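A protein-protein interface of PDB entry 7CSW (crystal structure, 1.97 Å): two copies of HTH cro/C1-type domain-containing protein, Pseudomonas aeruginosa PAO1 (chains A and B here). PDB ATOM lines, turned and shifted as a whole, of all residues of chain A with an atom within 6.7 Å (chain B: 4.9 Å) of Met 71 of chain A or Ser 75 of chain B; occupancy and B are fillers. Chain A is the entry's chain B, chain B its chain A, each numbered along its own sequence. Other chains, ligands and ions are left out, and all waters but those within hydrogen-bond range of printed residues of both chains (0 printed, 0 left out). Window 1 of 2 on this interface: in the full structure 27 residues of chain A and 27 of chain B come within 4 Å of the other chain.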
ATOM      1  N   ILE A  51      -6.279  30.742  19.113  1.00  0.00           N
ATOM      2  CA  ILE A  51      -5.086  30.320  18.386  1.00  0.00           C
ATOM      3  C   ILE A  51      -4.882  28.816  18.575  1.00  0.00           C
ATOM      4  O   ILE A  51      -4.701  28.339  19.697  1.00  0.00           O
ATOM      5  CB  ILE A  51      -3.854  31.125  18.829  1.00  0.00           C
ATOM      6  CG1 ILE A  51      -4.000  32.569  18.316  1.00  0.00           C
ATOM      7  CG2 ILE A  51      -2.581  30.480  18.293  1.00  0.00           C
ATOM      8  CD1 ILE A  51      -2.816  33.453  18.527  1.00  0.00           C
ATOM      9  N   SER A  52      -4.923  28.063  17.480  1.00  0.00           N
ATOM     10  CA  SER A  52      -4.653  26.636  17.527  1.00  0.00           C
ATOM     11  C   SER A  52      -3.151  26.383  17.613  1.00  0.00           C
ATOM     12  O   SER A  52      -2.330  27.273  17.371  1.00  0.00           O
ATOM     13  CB  SER A  52      -5.215  25.939  16.289  1.00  0.00           C
ATOM     14  OG  SER A  52      -4.439  26.313  15.159  1.00  0.00           O
ATOM     15  N   ALA A  53      -2.788  25.145  17.958  1.00  0.00           N
ATOM     16  CA  ALA A  53      -1.372  24.765  17.966  1.00  0.00           C
ATOM     17  C   ALA A  53      -0.736  24.992  16.597  1.00  0.00           C
ATOM     18  O   ALA A  53       0.393  25.493  16.496  1.00  0.00           O
ATOM     19  CB  ALA A  53      -1.221  23.299  18.391  1.00  0.00           C
ATOM     20  N   ASP A  54      -1.453  24.640  15.531  1.00  0.00           N
ATOM     21  CA  ASP A  54      -0.939  24.857  14.185  1.00  0.00           C
ATOM     22  C   ASP A  54      -0.682  26.339  13.928  1.00  0.00           C
ATOM     23  O   ASP A  54       0.388  26.721  13.427  1.00  0.00           O
ATOM     24  CB  ASP A  54      -1.927  24.271  13.172  1.00  0.00           C
ATOM     25  CG  ASP A  54      -1.477  24.442  11.741  1.00  0.00           C
ATOM     26  OD1 ASP A  54      -0.663  23.620  11.272  1.00  0.00           O
ATOM     27  OD2 ASP A  54      -1.953  25.386  11.084  1.00  0.00           O
ATOM     28  N   ALA A  56      -0.166  28.681  16.166  1.00  0.00           N
ATOM     29  CA  ALA A  56       0.932  29.127  17.018  1.00  0.00           C
ATOM     30  C   ALA A  56       2.285  28.890  16.347  1.00  0.00           C
ATOM     31  O   ALA A  56       3.175  29.747  16.404  1.00  0.00           O
ATOM     32  CB  ALA A  56       0.877  28.394  18.358  1.00  0.00           C
ATOM     33  N   ILE A  57       2.454  27.725  15.715  1.00  0.00           N
ATOM     34  CA  ILE A  57       3.696  27.435  15.000  1.00  0.00           C
ATOM     35  C   ILE A  57       3.878  28.392  13.831  1.00  0.00           C
ATOM     36  O   ILE A  57       4.975  28.940  13.621  1.00  0.00           O
ATOM     37  CB  ILE A  57       3.723  25.971  14.528  1.00  0.00           C
ATOM     38  CG1 ILE A  57       3.612  25.029  15.734  1.00  0.00           C
ATOM     39  CG2 ILE A  57       5.009  25.706  13.734  1.00  0.00           C
ATOM     40  CD1 ILE A  57       3.436  23.554  15.377  1.00  0.00           C
ATOM     41  N   SER A  66       8.654  33.049  19.765  1.00  0.00           N
ATOM     42  CA  SER A  66       8.351  31.755  20.367  1.00  0.00           C
ATOM     43  C   SER A  66       6.992  31.262  19.876  1.00  0.00           C
ATOM     44  O   SER A  66       6.028  32.032  19.803  1.00  0.00           O
ATOM     45  CB  SER A  66       8.346  31.897  21.890  1.00  0.00           C
ATOM     46  OG  SER A  66       7.825  30.735  22.512  1.00  0.00           O
ATOM     47  N   ALA A  67       6.912  29.979  19.516  1.00  0.00           N
ATOM     48  CA  ALA A  67       5.590  29.385  19.297  1.00  0.00           C
ATOM     49  C   ALA A  67       4.827  29.237  20.611  1.00  0.00           C
ATOM     50  O   ALA A  67       3.606  29.426  20.653  1.00  0.00           O
ATOM     51  CB  ALA A  67       5.711  28.026  18.609  1.00  0.00           C
ATOM     52  N   GLN A  68       5.526  28.870  21.688  1.00  0.00           N
ATOM     53  CA  GLN A  68       4.857  28.715  22.978  1.00  0.00           C
ATOM     54  C   GLN A  68       4.328  30.047  23.505  1.00  0.00           C
ATOM     55  O   GLN A  68       3.356  30.051  24.265  1.00  0.00           O
ATOM     56  CB  GLN A  68       5.804  28.057  23.988  1.00  0.00           C
ATOM     57  CG  GLN A  68       5.145  27.640  25.339  1.00  0.00           C
ATOM     58  CD  GLN A  68       4.219  26.413  25.251  1.00  0.00           C
ATOM     59  OE1 GLN A  68       4.564  25.384  24.655  1.00  0.00           O
ATOM     60  NE2 GLN A  68       3.039  26.516  25.876  1.00  0.00           N
ATOM     61  N   PHE A  69       4.922  31.172  23.090  1.00  0.00           N
ATOM     62  CA  PHE A  69       4.371  32.484  23.427  1.00  0.00           C
ATOM     63  C   PHE A  69       2.908  32.578  23.016  1.00  0.00           C
ATOM     64  O   PHE A  69       2.055  32.983  23.814  1.00  0.00           O
ATOM     65  CB  PHE A  69       5.204  33.590  22.767  1.00  0.00           C
ATOM     66  CG  PHE A  69       4.525  34.960  22.711  1.00  0.00           C
ATOM     67  CD1 PHE A  69       4.447  35.766  23.841  1.00  0.00           C
ATOM     68  CD2 PHE A  69       4.014  35.448  21.519  1.00  0.00           C
ATOM     69  CE1 PHE A  69       3.852  37.013  23.788  1.00  0.00           C
ATOM     70  CE2 PHE A  69       3.414  36.696  21.458  1.00  0.00           C
ATOM     71  CZ  PHE A  69       3.338  37.480  22.592  1.00  0.00           C
ATOM     72  N   TRP A  70       2.592  32.168  21.778  1.00  0.00           N
ATOM     73  CA  TRP A  70       1.199  32.188  21.329  1.00  0.00           C
ATOM     74  C   TRP A  70       0.348  31.163  22.074  1.00  0.00           C
ATOM     75  O   TRP A  70      -0.798  31.456  22.446  1.00  0.00           O
ATOM     76  CB  TRP A  70       1.132  31.954  19.825  1.00  0.00           C
ATOM     77  CG  TRP A  70       1.803  33.065  19.072  1.00  0.00           C
ATOM     78  CD1 TRP A  70       3.037  33.039  18.481  1.00  0.00           C
ATOM     79  CD2 TRP A  70       1.291  34.389  18.881  1.00  0.00           C
ATOM     80  NE1 TRP A  70       3.310  34.271  17.910  1.00  0.00           N
ATOM     81  CE2 TRP A  70       2.252  35.111  18.143  1.00  0.00           C
ATOM     82  CE3 TRP A  70       0.103  35.031  19.255  1.00  0.00           C
ATOM     83  CZ2 TRP A  70       2.058  36.451  17.761  1.00  0.00           C
ATOM     84  CZ3 TRP A  70      -0.091  36.353  18.873  1.00  0.00           C
ATOM     85  CH2 TRP A  70       0.883  37.044  18.130  1.00  0.00           C
ATOM     86  N   MET A  71       0.887  29.962  22.302  1.00  0.00           N
ATOM     87  CA  MET A  71       0.162  28.963  23.084  1.00  0.00           C
ATOM     88  C   MET A  71      -0.194  29.495  24.468  1.00  0.00           C
ATOM     89  O   MET A  71      -1.292  29.237  24.978  1.00  0.00           O
ATOM     90  CB  MET A  71       0.992  27.679  23.214  1.00  0.00           C
ATOM     91  CG  MET A  71       1.270  26.917  21.903  1.00  0.00           C
ATOM     92  SD  MET A  71      -0.216  26.326  21.059  1.00  0.00           S
ATOM     93  CE  MET A  71      -0.802  25.088  22.201  1.00  0.00           C
ATOM     94  N   ASN A  72       0.723  30.237  25.099  1.00  0.00           N
ATOM     95  CA  ASN A  72       0.485  30.707  26.465  1.00  0.00           C
ATOM     96  C   ASN A  72      -0.558  31.820  26.507  1.00  0.00           C
ATOM     97  O   ASN A  72      -1.393  31.864  27.425  1.00  0.00           O
ATOM     98  CB  ASN A  72       1.803  31.171  27.102  1.00  0.00           C
ATOM     99  CG  ASN A  72       2.757  29.998  27.392  1.00  0.00           C
ATOM    100  OD1 ASN A  72       2.329  28.839  27.466  1.00  0.00           O
ATOM    101  ND2 ASN A  72       4.053  30.301  27.555  1.00  0.00           N
ATOM    102  N   LEU A  73      -0.505  32.749  25.545  1.00  0.00           N
ATOM    103  CA  LEU A  73      -1.554  33.757  25.426  1.00  0.00           C
ATOM    104  C   LEU A  73      -2.923  33.097  25.339  1.00  0.00           C
ATOM    105  O   LEU A  73      -3.868  33.492  26.033  1.00  0.00           O
ATOM    106  CB  LEU A  73      -1.308  34.636  24.195  1.00  0.00           C
ATOM    107  CG  LEU A  73      -0.262  35.746  24.217  1.00  0.00           C
ATOM    108  CD1 LEU A  73      -0.187  36.451  22.838  1.00  0.00           C
ATOM    109  CD2 LEU A  73      -0.556  36.760  25.310  1.00  0.00           C
ATOM    110  N   GLN A  74      -3.039  32.065  24.506  1.00  0.00           N
ATOM    111  CA  GLN A  74      -4.320  31.389  24.336  1.00  0.00           C
ATOM    112  C   GLN A  74      -4.746  30.666  25.605  1.00  0.00           C
ATOM    113  O   GLN A  74      -5.904  30.766  26.029  1.00  0.00           O
ATOM    114  CB  GLN A  74      -4.253  30.390  23.182  1.00  0.00           C
ATOM    115  CG  GLN A  74      -5.607  29.757  22.907  1.00  0.00           C
ATOM    116  CD  GLN A  74      -6.640  30.820  22.565  1.00  0.00           C
ATOM    117  OE1 GLN A  74      -6.436  31.606  21.646  1.00  0.00           O
ATOM    118  NE2 GLN A  74      -7.729  30.873  23.326  1.00  0.00           N
ATOM    119  N   SER A  75      -3.834  29.903  26.209  1.00  0.00           N
ATOM    120  CA  SER A  75      -4.247  29.089  27.350  1.00  0.00           C
ATOM    121  C   SER A  75      -4.643  29.963  28.527  1.00  0.00           C
ATOM    122  O   SER A  75      -5.600  29.651  29.240  1.00  0.00           O
ATOM    123  CB  SER A  75      -3.141  28.117  27.757  1.00  0.00           C
ATOM    124  OG  SER A  75      -2.098  28.790  28.438  1.00  0.00           O
ATOM    125  N   GLU A  76      -3.931  31.064  28.742  1.00  0.00           N
ATOM    126  CA  GLU A  76      -4.315  31.976  29.817  1.00  0.00           C
ATOM    127  C   GLU A  76      -5.676  32.607  29.550  1.00  0.00           C
ATOM    128  O   GLU A  76      -6.509  32.723  30.459  1.00  0.00           O
ATOM    129  CB  GLU A  76      -3.245  33.047  29.990  1.00  0.00           C
ATOM    130  CG  GLU A  76      -1.960  32.524  30.624  1.00  0.00           C
ATOM    131  CD  GLU A  76      -0.835  33.553  30.612  1.00  0.00           C
ATOM    132  OE1 GLU A  76       0.335  33.168  30.370  1.00  0.00           O
ATOM    133  OE2 GLU A  76      -1.123  34.749  30.842  1.00  0.00           O
ATOM    134  N   MET B  71      -3.323  23.465  32.394  1.00  0.00           N
ATOM    135  CA  MET B  71      -3.351  24.149  31.103  1.00  0.00           C
ATOM    136  C   MET B  71      -1.984  24.099  30.430  1.00  0.00           C
ATOM    137  O   MET B  71      -1.892  23.904  29.214  1.00  0.00           O
ATOM    138  CB  MET B  71      -3.800  25.606  31.273  1.00  0.00           C
ATOM    139  CG  MET B  71      -5.247  25.799  31.747  1.00  0.00           C
ATOM    140  SD  MET B  71      -6.483  25.173  30.581  1.00  0.00           S
ATOM    141  CE  MET B  71      -6.320  26.345  29.251  1.00  0.00           C
ATOM    142  N   ASN B  72      -0.906  24.260  31.209  1.00  0.00           N
ATOM    143  CA  ASN B  72       0.435  24.300  30.624  1.00  0.00           C
ATOM    144  C   ASN B  72       0.887  22.919  30.163  1.00  0.00           C
ATOM    145  O   ASN B  72       1.542  22.793  29.121  1.00  0.00           O
ATOM    146  CB  ASN B  72       1.441  24.883  31.623  1.00  0.00           C
ATOM    147  CG  ASN B  72       1.188  26.366  31.919  1.00  0.00           C
ATOM    148  OD1 ASN B  72       0.532  27.071  31.144  1.00  0.00           O
ATOM    149  ND2 ASN B  72       1.711  26.840  33.054  1.00  0.00           N
ATOM    150  N   LEU B  73       0.579  21.876  30.939  1.00  0.00           N
ATOM    151  CA  LEU B  73       0.852  20.515  30.482  1.00  0.00           C
ATOM    152  C   LEU B  73       0.195  20.260  29.133  1.00  0.00           C
ATOM    153  O   LEU B  73       0.831  19.756  28.200  1.00  0.00           O
ATOM    154  CB  LEU B  73       0.357  19.498  31.513  1.00  0.00           C
ATOM    155  CG  LEU B  73       1.106  19.290  32.827  1.00  0.00           C
ATOM    156  CD1 LEU B  73       0.313  18.336  33.741  1.00  0.00           C
ATOM    157  CD2 LEU B  73       2.494  18.728  32.579  1.00  0.00           C
ATOM    158  N   GLN B  74      -1.082  20.626  29.008  1.00  0.00           N
ATOM    159  CA  GLN B  74      -1.809  20.403  27.762  1.00  0.00           C
ATOM    160  C   GLN B  74      -1.226  21.220  26.615  1.00  0.00           C
ATOM    161  O   GLN B  74      -1.027  20.701  25.511  1.00  0.00           O
ATOM    162  CB  GLN B  74      -3.286  20.749  27.940  1.00  0.00           C
ATOM    163  CG  GLN B  74      -4.097  20.449  26.695  1.00  0.00           C
ATOM    164  CD  GLN B  74      -3.994  18.981  26.338  1.00  0.00           C
ATOM    165  OE1 GLN B  74      -4.272  18.128  27.165  1.00  0.00           O
ATOM    166  NE2 GLN B  74      -3.561  18.681  25.119  1.00  0.00           N
ATOM    167  N   SER B  75      -0.960  22.508  26.851  1.00  0.00           N
ATOM    168  CA  SER B  75      -0.498  23.357  25.754  1.00  0.00           C
ATOM    169  C   SER B  75       0.869  22.914  25.259  1.00  0.00           C
ATOM    170  O   SER B  75       1.128  22.923  24.052  1.00  0.00           O
ATOM    171  CB  SER B  75      -0.461  24.825  26.177  1.00  0.00           C
ATOM    172  OG  SER B  75       0.688  25.091  26.955  1.00  0.00           O
ATOM    173  N   GLU B  76       1.744  22.488  26.172  1.00  0.00           N
ATOM    174  CA  GLU B  76       3.057  22.010  25.751  1.00  0.00           C
ATOM    175  C   GLU B  76       2.940  20.712  24.964  1.00  0.00           C
ATOM    176  O   GLU B  76       3.620  20.525  23.948  1.00  0.00           O
ATOM    177  CB  GLU B  76       3.957  21.831  26.966  1.00  0.00           C
ATOM    178  CG  GLU B  76       4.487  23.141  27.530  1.00  0.00           C
ATOM    179  CD  GLU B  76       4.878  23.023  29.001  1.00  0.00           C
ATOM    180  OE1 GLU B  76       5.175  24.068  29.633  1.00  0.00           O
ATOM    181  OE2 GLU B  76       4.872  21.884  29.526  1.00  0.00           O
ATOM    182  N   TYR B  77       2.076  19.801  25.419  1.00  0.00           N
ATOM    183  CA  TYR B  77       1.868  18.560  24.690  1.00  0.00           C
ATOM    184  C   TYR B  77       1.244  18.820  23.329  1.00  0.00           C
ATOM    185  O   TYR B  77       1.659  18.222  22.325  1.00  0.00           O
ATOM    186  CB  TYR B  77       0.981  17.621  25.507  1.00  0.00           C
ATOM    187  CG  TYR B  77       0.650  16.339  24.778  1.00  0.00           C
ATOM    188  CD1 TYR B  77       1.535  15.262  24.779  1.00  0.00           C
ATOM    189  CD2 TYR B  77      -0.546  16.207  24.082  1.00  0.00           C
ATOM    190  CE1 TYR B  77       1.226  14.081  24.110  1.00  0.00           C
ATOM    191  CE2 TYR B  77      -0.847  15.046  23.406  1.00  0.00           C
ATOM    192  CZ  TYR B  77       0.031  13.992  23.424  1.00  0.00           C
ATOM    193  OH  TYR B  77      -0.307  12.847  22.744  1.00  0.00           O
ATOM    194  N   SER B  78       0.239  19.706  23.278  1.00  0.00           N
ATOM    195  CA  SER B  78      -0.424  20.015  22.015  1.00  0.00           C
ATOM    196  C   SER B  78       0.550  20.622  21.023  1.00  0.00           C
ATOM    197  O   SER B  78       0.486  20.329  19.823  1.00  0.00           O
ATOM    198  CB  SER B  78      -1.589  20.974  22.249  1.00  0.00           C
ATOM    199  OG  SER B  78      -2.655  20.323  22.896  1.00  0.00           O
ATOM    200  N   LEU B  79       1.442  21.499  21.502  1.00  0.00           N
ATOM    201  CA  LEU B  79       2.399  22.150  20.611  1.00  0.00           C
ATOM    202  C   LEU B  79       3.412  21.148  20.068  1.00  0.00           C
ATOM    203  O   LEU B  79       3.699  21.137  18.867  1.00  0.00           O
ATOM    204  CB  LEU B  79       3.114  23.293  21.337  1.00  0.00           C
ATOM    205  CG  LEU B  79       4.251  23.948  20.540  1.00  0.00           C
ATOM    206  CD1 LEU B  79       3.711  24.564  19.247  1.00  0.00           C
ATOM    207  CD2 LEU B  79       4.999  24.992  21.394  1.00  0.00           C
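OG of Ser 75 of chain B lies within hydrogen-bond range of NE2 of Gln 68 of chain A, at 3.0 Å.
The side-chain hydroxyl (OG) of Ser 66 of chain A sits at hydrogen-bond distance from the backbone NH (N) of Gln 68 of chain A, at 3.1 Å.
The side-chain amide nitrogen (NE2) of Gln 68 of chain A lies within hydrogen-bond range of the side-chain amide oxygen (OD1) of Asn 72 of chain A (2.9 Å).
OG of Ser 75 of chain A lies within hydrogen-bond range of O of Asn 72 of chain A.
The side-chain hydroxyl (OG) of Ser 75 of chain B sits at hydrogen-bond distance from the backbone carbonyl oxygen (O) of Asn 72 of chain B (3.3 Å).
NE2 of Gln 74 of chain B sits at hydrogen-bond distance from OG of Ser 78 of chain B (2.9 Å).
Ala 53 of chain A touches Ser 78 of chain B (CB to O, 3.7 Å).
CG1 of Ile 57 of chain A touches CD1 of Leu 79 of chain B (3.5 Å).
Gln 68 of chain A touches Glu 76 of chain B.
OE1 of Gln 68 of chain A touches CD2 of Leu 79 of chain B (3.3 Å).
CE of Met 71 of chain A touches O of Ser 75 of chain B (3.4 Å).
Ser 75 of chain A touches Met 71 of chain B.
Of the printed residues of chain B, Ile 57 of chain A touches Leu 79 (3.5 Å).
Trp 70 of chain A touches none of the printed residues of chain B.
Printed residues of chain B within 4 Å of Met 71 of chain A: Ser 75 (3.4 Å).
Printed residues of chain B within 4 Å of Ser 75 of chain A: Met 71.
Of the printed residues of chain A, Met 71 of chain B touches Ser 75 (3.4 Å).
Gln 74 of chain B touches none of the printed residues of chain A.
Ser 75 of chain B touches two residues of chain A.
Of the printed residues of chain A, Glu 76 of chain B touches Gln 68 (3.6 Å).
Of the printed residues of chain A, Leu 79 of chain B touches Ile 57 (3.5 Å) and Gln 68 (3.3 Å).
The nearest residue of chain A that does not touch Ser 75 of chain B is Asn 72 of chain A (4.1 Å).
The nearest printed residue of chain A that does not touch Ser 78 of chain B is Met 71 of chain A (4.2 Å).
Printed residues of chain A that touch a printed residue of chain B: Ala 53, Ile 57, Gln 68, Met 71 and Ser 75.
Hydrophobic or aromatic side chains of chain A within 4 Å of the printed part of chain B: Ala 53, Ile 57 and Met 71.
Of the 9 printed residues of chain B, 5 touch a printed residue of chain A.
Printed residues of chain B that touch a printed residue of chain A: Met 71, Ser 75, Glu 76, Ser 78 and Leu 79.
Hydrophobic or aromatic side chains of chain B that line the printed part of chain A: Met 71 and Leu 79.
Met 71 of chain A touches Ser 75 of chain B, and with the chains exchanged Ser 75 of chain A touches Met 71 of chain B.
Positions printed for both chains: 71, 72, 73, 74, 75 and 76.
Of the 7 pairs that touch across the chains among the printed residues, 2 have their exchanged pair printed and touching as well.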
